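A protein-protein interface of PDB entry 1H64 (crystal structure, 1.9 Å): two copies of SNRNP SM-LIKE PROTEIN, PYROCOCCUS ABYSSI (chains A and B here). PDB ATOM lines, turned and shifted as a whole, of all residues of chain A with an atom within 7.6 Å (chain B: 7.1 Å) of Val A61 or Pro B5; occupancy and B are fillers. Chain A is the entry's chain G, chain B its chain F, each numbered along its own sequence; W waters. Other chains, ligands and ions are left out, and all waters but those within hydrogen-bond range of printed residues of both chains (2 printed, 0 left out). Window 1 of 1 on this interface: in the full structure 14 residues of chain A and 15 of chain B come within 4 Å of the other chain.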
ATOM      1  N   PHE A  27      27.806 -16.065   0.299  1.00  0.00           N
ATOM      2  CA  PHE A  27      26.441 -16.534   0.224  1.00  0.00           C
ATOM      3  C   PHE A  27      25.760 -15.533  -0.693  1.00  0.00           C
ATOM      4  O   PHE A  27      26.115 -14.345  -0.698  1.00  0.00           O
ATOM      5  CB  PHE A  27      25.742 -16.500   1.596  1.00  0.00           C
ATOM      6  CG  PHE A  27      26.115 -17.633   2.507  1.00  0.00           C
ATOM      7  CD1 PHE A  27      26.942 -17.419   3.606  1.00  0.00           C
ATOM      8  CD2 PHE A  27      25.620 -18.908   2.287  1.00  0.00           C
ATOM      9  CE1 PHE A  27      27.267 -18.461   4.472  1.00  0.00           C
ATOM     10  CE2 PHE A  27      25.940 -19.963   3.149  1.00  0.00           C
ATOM     11  CZ  PHE A  27      26.762 -19.738   4.242  1.00  0.00           C
ATOM     12  N   ILE A  32      15.610 -11.075   3.037  1.00  0.00           N
ATOM     13  CA  ILE A  32      14.234 -10.982   3.512  1.00  0.00           C
ATOM     14  C   ILE A  32      14.158 -10.490   4.960  1.00  0.00           C
ATOM     15  O   ILE A  32      13.060 -10.345   5.519  1.00  0.00           O
ATOM     16  CB  ILE A  32      13.506 -12.342   3.395  1.00  0.00           C
ATOM     17  CG1 ILE A  32      14.251 -13.408   4.204  1.00  0.00           C
ATOM     18  CG2 ILE A  32      13.417 -12.761   1.908  1.00  0.00           C
ATOM     19  CD1 ILE A  32      13.495 -14.706   4.333  1.00  0.00           C
ATOM     20  N   GLY A  33      15.320 -10.227   5.559  1.00  0.00           N
ATOM     21  CA  GLY A  33      15.355  -9.755   6.937  1.00  0.00           C
ATOM     22  C   GLY A  33      16.756  -9.432   7.440  1.00  0.00           C
ATOM     23  O   GLY A  33      17.757  -9.879   6.877  1.00  0.00           O
ATOM     24  N   TYR A  34      16.828  -8.654   8.514  1.00  0.00           N
ATOM     25  CA  TYR A  34      18.115  -8.270   9.088  1.00  0.00           C
ATOM     26  C   TYR A  34      17.880  -7.589  10.429  1.00  0.00           C
ATOM     27  O   TYR A  34      16.738  -7.261  10.762  1.00  0.00           O
ATOM     28  CB  TYR A  34      18.836  -7.294   8.161  1.00  0.00           C
ATOM     29  CG  TYR A  34      18.175  -5.927   8.103  1.00  0.00           C
ATOM     30  CD1 TYR A  34      18.489  -4.935   9.038  1.00  0.00           C
ATOM     31  CD2 TYR A  34      17.200  -5.640   7.145  1.00  0.00           C
ATOM     32  CE1 TYR A  34      17.845  -3.695   9.023  1.00  0.00           C
ATOM     33  CE2 TYR A  34      16.553  -4.401   7.118  1.00  0.00           C
ATOM     34  CZ  TYR A  34      16.878  -3.437   8.062  1.00  0.00           C
ATOM     35  OH  TYR A  34      16.223  -2.224   8.064  1.00  0.00           O
ATOM     36  N   ASP A  35      18.955  -7.407  11.197  1.00  0.00           N
ATOM     37  CA  ASP A  35      18.859  -6.714  12.478  1.00  0.00           C
ATOM     38  C   ASP A  35      20.023  -5.752  12.650  1.00  0.00           C
ATOM     39  O   ASP A  35      20.910  -5.692  11.810  1.00  0.00           O
ATOM     40  CB  ASP A  35      18.761  -7.701  13.647  1.00  0.00           C
ATOM     41  CG  ASP A  35      20.000  -8.537  13.831  1.00  0.00           C
ATOM     42  OD1 ASP A  35      19.854  -9.621  14.438  1.00  0.00           O
ATOM     43  OD2 ASP A  35      21.101  -8.124  13.398  1.00  0.00           O
ATOM     44  N   ILE A  36      19.998  -4.978  13.735  1.00  0.00           N
ATOM     45  CA  ILE A  36      21.028  -3.990  14.006  1.00  0.00           C
ATOM     46  C   ILE A  36      22.457  -4.527  14.091  1.00  0.00           C
ATOM     47  O   ILE A  36      23.418  -3.782  13.914  1.00  0.00           O
ATOM     48  CB  ILE A  36      20.676  -3.205  15.307  1.00  0.00           C
ATOM     49  CG1 ILE A  36      21.758  -2.166  15.619  1.00  0.00           C
ATOM     50  CG2 ILE A  36      20.549  -4.171  16.474  1.00  0.00           C
ATOM     51  CD1 ILE A  36      22.116  -1.264  14.451  1.00  0.00           C
ATOM     52  N   LEU A  38      23.568  -6.550  12.083  1.00  0.00           N
ATOM     53  CA  LEU A  38      23.854  -6.935  10.703  1.00  0.00           C
ATOM     54  C   LEU A  38      23.801  -8.453  10.475  1.00  0.00           C
ATOM     55  O   LEU A  38      24.456  -8.990   9.563  1.00  0.00           O
ATOM     56  CB  LEU A  38      25.193  -6.366  10.238  1.00  0.00           C
ATOM     57  CG  LEU A  38      25.193  -4.841  10.031  1.00  0.00           C
ATOM     58  CD1 LEU A  38      26.526  -4.378   9.495  1.00  0.00           C
ATOM     59  CD2 LEU A  38      24.088  -4.462   9.058  1.00  0.00           C
ATOM     60  N   ASN A  39      23.041  -9.148  11.326  1.00  0.00           N
ATOM     61  CA  ASN A  39      22.794 -10.573  11.130  1.00  0.00           C
ATOM     62  C   ASN A  39      21.770 -10.492   9.993  1.00  0.00           C
ATOM     63  O   ASN A  39      20.953  -9.568   9.984  1.00  0.00           O
ATOM     64  CB  ASN A  39      22.110 -11.201  12.341  1.00  0.00           C
ATOM     65  CG  ASN A  39      22.986 -11.192  13.569  1.00  0.00           C
ATOM     66  OD1 ASN A  39      24.187 -11.415  13.476  1.00  0.00           O
ATOM     67  ND2 ASN A  39      22.384 -10.946  14.729  1.00  0.00           N
ATOM     68  N   VAL A  40      21.795 -11.423   9.037  1.00  0.00           N
ATOM     69  CA  VAL A  40      20.832 -11.334   7.932  1.00  0.00           C
ATOM     70  C   VAL A  40      20.143 -12.649   7.603  1.00  0.00           C
ATOM     71  O   VAL A  40      20.651 -13.732   7.922  1.00  0.00           O
ATOM     72  CB  VAL A  40      21.508 -10.785   6.628  1.00  0.00           C
ATOM     73  CG1 VAL A  40      22.038  -9.376   6.865  1.00  0.00           C
ATOM     74  CG2 VAL A  40      22.636 -11.697   6.188  1.00  0.00           C
ATOM     75  N   VAL A  41      18.972 -12.549   6.979  1.00  0.00           N
ATOM     76  CA  VAL A  41      18.210 -13.731   6.594  1.00  0.00           C
ATOM     77  C   VAL A  41      18.063 -13.695   5.079  1.00  0.00           C
ATOM     78  O   VAL A  41      17.638 -12.684   4.523  1.00  0.00           O
ATOM     79  CB  VAL A  41      16.814 -13.729   7.215  1.00  0.00           C
ATOM     80  CG1 VAL A  41      16.119 -15.071   6.934  1.00  0.00           C
ATOM     81  CG2 VAL A  41      16.929 -13.494   8.724  1.00  0.00           C
ATOM     82  N   LEU A  42      18.434 -14.792   4.432  1.00  0.00           N
ATOM     83  CA  LEU A  42      18.360 -14.901   2.979  1.00  0.00           C
ATOM     84  C   LEU A  42      17.456 -16.059   2.585  1.00  0.00           C
ATOM     85  O   LEU A  42      17.459 -17.101   3.246  1.00  0.00           O
ATOM     86  CB  LEU A  42      19.750 -15.162   2.393  1.00  0.00           C
ATOM     87  CG  LEU A  42      20.935 -14.240   2.697  1.00  0.00           C
ATOM     88  CD1 LEU A  42      22.136 -14.742   1.939  1.00  0.00           C
ATOM     89  CD2 LEU A  42      20.638 -12.812   2.295  1.00  0.00           C
ATOM     90  N   TYR A  57      20.199 -23.245  -0.002  1.00  0.00           N
ATOM     91  CA  TYR A  57      19.333 -23.300   1.165  1.00  0.00           C
ATOM     92  C   TYR A  57      18.048 -22.582   0.839  1.00  0.00           C
ATOM     93  O   TYR A  57      18.067 -21.559   0.158  1.00  0.00           O
ATOM     94  CB  TYR A  57      20.007 -22.609   2.362  1.00  0.00           C
ATOM     95  CG  TYR A  57      21.453 -22.995   2.581  1.00  0.00           C
ATOM     96  CD1 TYR A  57      22.481 -22.343   1.903  1.00  0.00           C
ATOM     97  CD2 TYR A  57      21.793 -23.995   3.485  1.00  0.00           C
ATOM     98  CE1 TYR A  57      23.807 -22.677   2.128  1.00  0.00           C
ATOM     99  CE2 TYR A  57      23.112 -24.335   3.715  1.00  0.00           C
ATOM    100  CZ  TYR A  57      24.115 -23.669   3.031  1.00  0.00           C
ATOM    101  OH  TYR A  57      25.420 -24.018   3.252  1.00  0.00           O
ATOM    102  N   LYS A  59      16.295 -21.203   3.052  1.00  0.00           N
ATOM    103  CA  LYS A  59      16.342 -20.036   3.945  1.00  0.00           C
ATOM    104  C   LYS A  59      17.518 -20.195   4.909  1.00  0.00           C
ATOM    105  O   LYS A  59      17.726 -21.267   5.454  1.00  0.00           O
ATOM    106  CB  LYS A  59      15.047 -19.934   4.740  1.00  0.00           C
ATOM    107  CG  LYS A  59      14.982 -18.746   5.691  1.00  0.00           C
ATOM    108  CD  LYS A  59      13.857 -17.827   5.322  1.00  0.00           C
ATOM    109  CE  LYS A  59      12.531 -18.561   5.366  1.00  0.00           C
ATOM    110  NZ  LYS A  59      11.405 -17.679   5.009  1.00  0.00           N
ATOM    111  N   ILE A  60      18.275 -19.123   5.125  1.00  0.00           N
ATOM    112  CA  ILE A  60      19.425 -19.199   6.020  1.00  0.00           C
ATOM    113  C   ILE A  60      19.627 -17.890   6.797  1.00  0.00           C
ATOM    114  O   ILE A  60      19.438 -16.805   6.256  1.00  0.00           O
ATOM    115  CB  ILE A  60      20.705 -19.548   5.214  1.00  0.00           C
ATOM    116  CG1 ILE A  60      21.866 -19.841   6.163  1.00  0.00           C
ATOM    117  CG2 ILE A  60      21.053 -18.420   4.248  1.00  0.00           C
ATOM    118  CD1 ILE A  60      23.084 -20.404   5.460  1.00  0.00           C
ATOM    119  N   VAL A  61      19.981 -18.008   8.074  1.00  0.00           N
ATOM    120  CA  VAL A  61      20.221 -16.831   8.917  1.00  0.00           C
ATOM    121  C   VAL A  61      21.737 -16.814   9.099  1.00  0.00           C
ATOM    122  O   VAL A  61      22.311 -17.783   9.598  1.00  0.00           O
ATOM    123  CB  VAL A  61      19.528 -16.966  10.297  1.00  0.00           C
ATOM    124  CG1 VAL A  61      19.797 -15.714  11.143  1.00  0.00           C
ATOM    125  CG2 VAL A  61      18.021 -17.169  10.113  1.00  0.00           C
ATOM    126  N   ILE A  62      22.372 -15.731   8.664  1.00  0.00           N
ATOM    127  CA  ILE A  62      23.823 -15.579   8.741  1.00  0.00           C
ATOM    128  C   ILE A  62      24.185 -14.583   9.859  1.00  0.00           C
ATOM    129  O   ILE A  62      23.562 -13.534   9.958  1.00  0.00           O
ATOM    130  CB  ILE A  62      24.358 -15.031   7.402  1.00  0.00           C
ATOM    131  CG1 ILE A  62      23.975 -15.996   6.269  1.00  0.00           C
ATOM    132  CG2 ILE A  62      25.866 -14.866   7.450  1.00  0.00           C
ATOM    133  CD1 ILE A  62      24.306 -15.491   4.866  1.00  0.00           C
ATOM    134  N   ARG A  63      25.175 -14.905  10.691  1.00  0.00           N
ATOM    135  CA  ARG A  63      25.549 -13.972  11.773  1.00  0.00           C
ATOM    136  C   ARG A  63      26.494 -12.888  11.273  1.00  0.00           C
ATOM    137  O   ARG A  63      27.506 -13.165  10.635  1.00  0.00           O
ATOM    138  CB  ARG A  63      26.159 -14.732  12.965  1.00  0.00           C
ATOM    139  CG  ARG A  63      25.126 -15.500  13.781  1.00  0.00           C
ATOM    140  CD  ARG A  63      25.746 -16.163  15.010  1.00  0.00           C
ATOM    141  NE  ARG A  63      26.338 -15.201  15.944  1.00  0.00           N
ATOM    142  CZ  ARG A  63      27.645 -14.969  16.066  1.00  0.00           C
ATOM    143  NH1 ARG A  63      28.535 -15.611  15.312  1.00  0.00           N
ATOM    144  NH2 ARG A  63      28.074 -14.103  16.975  1.00  0.00           N
ATOM    145  N   GLY A  64      26.154 -11.633  11.557  1.00  0.00           N
ATOM    146  CA  GLY A  64      26.988 -10.528  11.102  1.00  0.00           C
ATOM    147  C   GLY A  64      28.450 -10.527  11.529  1.00  0.00           C
ATOM    148  O   GLY A  64      29.292  -9.971  10.835  1.00  0.00           O
ATOM    149  N   GLU B   3      11.427 -10.891   7.555  1.00  0.00           N
ATOM    150  CA  GLU B   3      11.558 -11.882   8.661  1.00  0.00           C
ATOM    151  C   GLU B   3      12.906 -11.684   9.328  1.00  0.00           C
ATOM    152  O   GLU B   3      13.940 -12.047   8.771  1.00  0.00           O
ATOM    153  CB  GLU B   3      11.490 -13.298   8.108  1.00  0.00           C
ATOM    154  CG  GLU B   3      10.288 -13.576   7.235  1.00  0.00           C
ATOM    155  CD  GLU B   3      10.269 -15.006   6.752  1.00  0.00           C
ATOM    156  OE1 GLU B   3       9.307 -15.388   6.050  1.00  0.00           O
ATOM    157  OE2 GLU B   3      11.222 -15.748   7.079  1.00  0.00           O
ATOM    158  N   ARG B   4      12.901 -11.110  10.519  1.00  0.00           N
ATOM    159  CA  ARG B   4      14.150 -10.883  11.212  1.00  0.00           C
ATOM    160  C   ARG B   4      14.753 -12.194  11.697  1.00  0.00           C
ATOM    161  O   ARG B   4      14.046 -13.184  11.918  1.00  0.00           O
ATOM    162  CB  ARG B   4      13.940  -9.918  12.382  1.00  0.00           C
ATOM    163  CG  ARG B   4      13.670  -8.480  11.928  1.00  0.00           C
ATOM    164  CD  ARG B   4      14.356  -7.480  12.858  1.00  0.00           C
ATOM    165  NE  ARG B   4      14.404  -6.125  12.309  1.00  0.00           N
ATOM    166  CZ  ARG B   4      15.005  -5.097  12.907  1.00  0.00           C
ATOM    167  NH1 ARG B   4      15.609  -5.267  14.076  1.00  0.00           N
ATOM    168  NH2 ARG B   4      15.004  -3.898  12.336  1.00  0.00           N
ATOM    169  N   PRO B   5      16.081 -12.218  11.864  1.00  0.00           N
ATOM    170  CA  PRO B   5      16.798 -13.410  12.326  1.00  0.00           C
ATOM    171  C   PRO B   5      16.107 -14.168  13.463  1.00  0.00           C
ATOM    172  O   PRO B   5      15.915 -15.386  13.387  1.00  0.00           O
ATOM    173  CB  PRO B   5      18.155 -12.842  12.729  1.00  0.00           C
ATOM    174  CG  PRO B   5      18.364 -11.793  11.658  1.00  0.00           C
ATOM    175  CD  PRO B   5      17.018 -11.103  11.608  1.00  0.00           C
ATOM    176  N   LEU B   6      15.726 -13.459  14.520  1.00  0.00           N
ATOM    177  CA  LEU B   6      15.072 -14.110  15.651  1.00  0.00           C
ATOM    178  C   LEU B   6      13.688 -14.665  15.329  1.00  0.00           C
ATOM    179  O   LEU B   6      13.251 -15.649  15.945  1.00  0.00           O
ATOM    180  CB  LEU B   6      14.977 -13.148  16.843  1.00  0.00           C
ATOM    181  CG  LEU B   6      16.241 -12.982  17.688  1.00  0.00           C
ATOM    182  CD1 LEU B   6      16.583 -14.314  18.341  1.00  0.00           C
ATOM    183  CD2 LEU B   6      17.399 -12.500  16.820  1.00  0.00           C
ATOM    184  N   ASP B   7      12.990 -14.037  14.384  1.00  0.00           N
ATOM    185  CA  ASP B   7      11.652 -14.498  13.997  1.00  0.00           C
ATOM    186  C   ASP B   7      11.772 -15.877  13.347  1.00  0.00           C
ATOM    187  O   ASP B   7      11.000 -16.796  13.637  1.00  0.00           O
ATOM    188  CB  ASP B   7      11.021 -13.532  12.996  1.00  0.00           C
ATOM    189  CG  ASP B   7      10.569 -12.236  13.635  1.00  0.00           C
ATOM    190  OD1 ASP B   7      10.494 -11.219  12.911  1.00  0.00           O
ATOM    191  OD2 ASP B   7      10.271 -12.245  14.851  1.00  0.00           O
ATOM    192  N   VAL B   8      12.741 -15.995  12.451  1.00  0.00           N
ATOM    193  CA  VAL B   8      12.999 -17.244  11.752  1.00  0.00           C
ATOM    194  C   VAL B   8      13.385 -18.353  12.726  1.00  0.00           C
ATOM    195  O   VAL B   8      12.933 -19.482  12.600  1.00  0.00           O
ATOM    196  CB  VAL B   8      14.139 -17.064  10.742  1.00  0.00           C
ATOM    197  CG1 VAL B   8      14.535 -18.413  10.158  1.00  0.00           C
ATOM    198  CG2 VAL B   8      13.698 -16.117   9.646  1.00  0.00           C
ATOM    199  N   ILE B   9      14.229 -18.030  13.698  1.00  0.00           N
ATOM    200  CA  ILE B   9      14.672 -19.019  14.672  1.00  0.00           C
ATOM    201  C   ILE B   9      13.501 -19.444  15.541  1.00  0.00           C
ATOM    202  O   ILE B   9      13.294 -20.631  15.819  1.00  0.00           O
ATOM    203  CB  ILE B   9      15.817 -18.423  15.558  1.00  0.00           C
ATOM    204  CG1 ILE B   9      17.021 -18.118  14.676  1.00  0.00           C
ATOM    205  CG2 ILE B   9      16.184 -19.371  16.676  1.00  0.00           C
ATOM    206  CD1 ILE B   9      18.147 -17.403  15.388  1.00  0.00           C
ATOM    207  N   HIS B  10      12.716 -18.464  15.964  1.00  0.00           N
ATOM    208  CA  HIS B  10      11.573 -18.754  16.803  1.00  0.00           C
ATOM    209  C   HIS B  10      10.621 -19.682  16.043  1.00  0.00           C
ATOM    210  O   HIS B  10      10.139 -20.671  16.584  1.00  0.00           O
ATOM    211  CB  HIS B  10      10.846 -17.459  17.172  1.00  0.00           C
ATOM    212  CG  HIS B  10       9.626 -17.688  17.996  1.00  0.00           C
ATOM    213  ND1 HIS B  10       9.686 -18.106  19.307  1.00  0.00           N
ATOM    214  CD2 HIS B  10       8.313 -17.641  17.672  1.00  0.00           C
ATOM    215  CE1 HIS B  10       8.460 -18.309  19.756  1.00  0.00           C
ATOM    216  NE2 HIS B  10       7.609 -18.036  18.782  1.00  0.00           N
ATOM    217  N   ARG B  11      10.374 -19.348  14.781  1.00  0.00           N
ATOM    218  CA  ARG B  11       9.475 -20.121  13.938  1.00  0.00           C
ATOM    219  C   ARG B  11       9.980 -21.546  13.738  1.00  0.00           C
ATOM    220  O   ARG B  11       9.203 -22.453  13.415  1.00  0.00           O
ATOM    221  CB  ARG B  11       9.333 -19.437  12.575  1.00  0.00           C
ATOM    222  CG  ARG B  11       7.910 -19.388  12.044  1.00  0.00           C
ATOM    223  CD  ARG B  11       7.882 -18.880  10.604  1.00  0.00           C
ATOM    224  NE  ARG B  11       8.518 -17.569  10.448  1.00  0.00           N
ATOM    225  CZ  ARG B  11       8.035 -16.429  10.937  1.00  0.00           C
ATOM    226  NH1 ARG B  11       6.898 -16.419  11.624  1.00  0.00           N
ATOM    227  NH2 ARG B  11       8.691 -15.293  10.739  1.00  0.00           N
ATOM    228  N   LEU B  18      19.890 -26.746  10.541  1.00  0.00           N
ATOM    229  CA  LEU B  18      21.295 -26.981  10.250  1.00  0.00           C
ATOM    230  C   LEU B  18      22.080 -25.810  10.849  1.00  0.00           C
ATOM    231  O   LEU B  18      21.853 -24.665  10.468  1.00  0.00           O
ATOM    232  CB  LEU B  18      21.530 -27.016   8.743  1.00  0.00           C
ATOM    233  CG  LEU B  18      23.000 -27.129   8.344  1.00  0.00           C
ATOM    234  CD1 LEU B  18      23.551 -28.454   8.840  1.00  0.00           C
ATOM    235  CD2 LEU B  18      23.148 -27.013   6.834  1.00  0.00           C
ATOM    236  N   LEU B  38      21.782 -16.117  20.306  1.00  0.00           N
ATOM    237  CA  LEU B  38      21.824 -17.146  19.277  1.00  0.00           C
ATOM    238  C   LEU B  38      22.498 -18.441  19.745  1.00  0.00           C
ATOM    239  O   LEU B  38      23.018 -19.212  18.929  1.00  0.00           O
ATOM    240  CB  LEU B  38      22.484 -16.637  17.995  1.00  0.00           C
ATOM    241  CG  LEU B  38      21.564 -15.978  16.967  1.00  0.00           C
ATOM    242  CD1 LEU B  38      20.755 -14.887  17.620  1.00  0.00           C
ATOM    243  CD2 LEU B  38      22.382 -15.434  15.829  1.00  0.00           C
ATOM    244  N   VAL B  67      28.854 -19.738  15.810  1.00  0.00           N
ATOM    245  CA  VAL B  67      27.965 -20.043  14.695  1.00  0.00           C
ATOM    246  C   VAL B  67      28.131 -19.124  13.497  1.00  0.00           C
ATOM    247  O   VAL B  67      28.164 -17.895  13.638  1.00  0.00           O
ATOM    248  CB  VAL B  67      26.484 -19.998  15.134  1.00  0.00           C
ATOM    249  CG1 VAL B  67      25.576 -20.194  13.916  1.00  0.00           C
ATOM    250  CG2 VAL B  67      26.201 -21.103  16.171  1.00  0.00           C
ATOM    251  N   LEU B  68      28.259 -19.725  12.313  1.00  0.00           N
ATOM    252  CA  LEU B  68      28.350 -18.949  11.080  1.00  0.00           C
ATOM    253  C   LEU B  68      26.923 -18.722  10.569  1.00  0.00           C
ATOM    254  O   LEU B  68      26.556 -17.613  10.212  1.00  0.00           O
ATOM    255  CB  LEU B  68      29.162 -19.687  10.000  1.00  0.00           C
ATOM    256  CG  LEU B  68      29.123 -19.101   8.571  1.00  0.00           C
ATOM    257  CD1 LEU B  68      29.750 -17.711   8.545  1.00  0.00           C
ATOM    258  CD2 LEU B  68      29.861 -20.023   7.607  1.00  0.00           C
ATOM    259  N   ALA B  69      26.107 -19.779  10.549  1.00  0.00           N
ATOM    260  CA  ALA B  69      24.738 -19.638  10.048  1.00  0.00           C
ATOM    261  C   ALA B  69      23.829 -20.727  10.559  1.00  0.00           C
ATOM    262  O   ALA B  69      24.300 -21.754  11.029  1.00  0.00           O
ATOM    263  CB  ALA B  69      24.743 -19.650   8.522  1.00  0.00           C
ATOM    264  N   ILE B  70      22.520 -20.485  10.469  1.00  0.00           N
ATOM    265  CA  ILE B  70      21.509 -21.448  10.910  1.00  0.00           C
ATOM    266  C   ILE B  70      20.460 -21.521   9.816  1.00  0.00           C
ATOM    267  O   ILE B  70      19.937 -20.488   9.389  1.00  0.00           O
ATOM    268  CB  ILE B  70      20.801 -20.985  12.192  1.00  0.00           C
ATOM    269  CG1 ILE B  70      21.808 -20.867  13.335  1.00  0.00           C
ATOM    270  CG2 ILE B  70      19.692 -21.994  12.558  1.00  0.00           C
ATOM    271  CD1 ILE B  70      21.204 -20.328  14.607  1.00  0.00           C
ATOM    272  N   SER B  71      20.147 -22.732   9.360  1.00  0.00           N
ATOM    273  CA  SER B  71      19.164 -22.888   8.294  1.00  0.00           C
ATOM    274  C   SER B  71      18.055 -23.873   8.652  1.00  0.00           C
ATOM    275  O   SER B  71      18.332 -25.029   8.962  1.00  0.00           O
ATOM    276  CB  SER B  71      19.858 -23.371   7.017  1.00  0.00           C
ATOM    277  OG  SER B  71      18.932 -23.697   5.990  1.00  0.00           O
ATOM    278  N   PRO B  72      16.789 -23.416   8.655  1.00  0.00           N
ATOM    279  CA  PRO B  72      15.713 -24.363   8.975  1.00  0.00           C
ATOM    280  C   PRO B  72      15.708 -25.253   7.728  1.00  0.00           C
ATOM    281  O   PRO B  72      15.538 -24.746   6.614  1.00  0.00           O
ATOM    282  CB  PRO B  72      14.464 -23.480   9.033  1.00  0.00           C
ATOM    283  CG  PRO B  72      14.993 -22.083   9.223  1.00  0.00           C
ATOM    284  CD  PRO B  72      16.246 -22.076   8.392  1.00  0.00           C
HETATM  285  O   HOH W   1      16.043 -23.912   4.374  1.00  0.00           O
HETATM  286  O   HOH W   2      11.928  -8.434   7.088  1.00  0.00           O
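Among the printed residues, merely in contact across the chains: Val A61 with Ala B69, Gly A33 with Glu B3, Val A41 with Glu B3, Lys A59 with Pro B72, Arg A63 with Leu B38, Val A41 with Pro B5, Ile A60 with Ala B69, Ile A60 with Ile B70, Val A61 with Pro B5, Val A61 with Val B8, Ile A62 with Leu B68, Val A41 with Val B8, Asn A39 with Pro B5, Tyr A34 with Pro B5, Tyr A57 with Ser B71, Asp A35 with Pro B5, Asp A35 with Arg B4 and Val A41 with Arg B4.
Position printed for both chains: 38.
Of the 25 pairs that touch across the chains among the printed residues, none has its exchanged pair printed and touching as well.
OD1 of Asp B7 sits at hydrogen-bond distance from N of Arg B4, 3.4 Å away.
The backbone carbonyl oxygen (O) of Ser B71 sits at hydrogen-bond distance from the backbone NH (N) of Leu B18, 2.8 Å away.
The backbone carbonyl oxygen (O) of Val A41 lies within hydrogen-bond range of the backbone NH (N) of Ile A32 (3.0 Å).
The side-chain carboxylate (OD2) of Asp A35 sits at hydrogen-bond distance from the backbone NH (N) of Leu A38 (3.2 Å).
OD1 of Asp A35 lies within hydrogen-bond range of ND2 of Asn A39, 2.9 Å away.
O of Leu A42 sits at hydrogen-bond distance from N of Ile A60, at 2.9 Å.
The backbone carbonyl oxygen of Ile A32 lies within hydrogen-bond range of the backbone NH of Glu B3.
OE2 of Glu B3 is in salt-bridge range of NZ of Lys A59 (2.8 Å).
The guanidinium group of Arg B4 is in hydrogen-bond range of the backbone carbonyl oxygen of Tyr A34 (3.0 Å).
O of Val B67 lies within hydrogen-bond range of NH1 of Arg A63, 2.9 Å away.
The backbone carbonyl oxygen of Leu B68 is in hydrogen-bond range of the backbone NH of Arg A63, 3.1 Å away.
The backbone carbonyl oxygen of Ile B70 is in hydrogen-bond range of the backbone NH of Val A61 (2.8 Å).
OG of Ser B71 is in hydrogen-bond range of O of Lys A59 (2.8 Å).
Water W1 lies within hydrogen-bond range of O of Pro B72, N of Lys A59 and OG of Ser B71.
Water W2 lies within hydrogen-bond range of the backbone NH of Glu B3 (2.6 Å) and the backbone carbonyl oxygen of Ile A32 (2.7 Å).
Printed residues of chain A that touch a printed residue of chain B: Ile A32, Gly A33, Tyr A34, Asp A35, Asn A39, Val A41, Tyr A57, Lys A59, Ile A60, Val A61, Ile A62 and Arg A63.
Hydrophobic or aromatic side chains of chain A that line the printed part of chain B: Ile A32, Val A41, Tyr A57, Ile A60, Val A61 and Ile A62.
Hydrophobic or aromatic side chains of chain B within 4 Å of the printed part of chain A: Pro B5, Val B8, Leu B38, Val B67, Ala B69 and Pro B72.
Among the printed residues, Asp or Glu carboxylates within 4 Å of a Lys or Arg side-chain nitrogen of the other chain: Lys A59 with Glu B3 (2.8 Å).
Of the printed residues of chain B, Val A61 touches Pro B5 (3.7 Å), Val B8 (3.7 Å), Ala B69 (3.1 Å) and Ile B70 (2.8 Å).
Of the printed residues of chain A, Pro B5 touches Tyr A34 (3.8 Å), Asp A35 (3.8 Å), Asn A39 (3.8 Å), Val A41 (3.5 Å) and Val A61 (3.7 Å).
Printed residues of chain B within 4 Å of Asn A39: Pro B5 (3.8 Å).
Of the printed residues of chain A, Val B67 touches Arg A63.
Phe A27 touches none of the printed residues of chain B.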
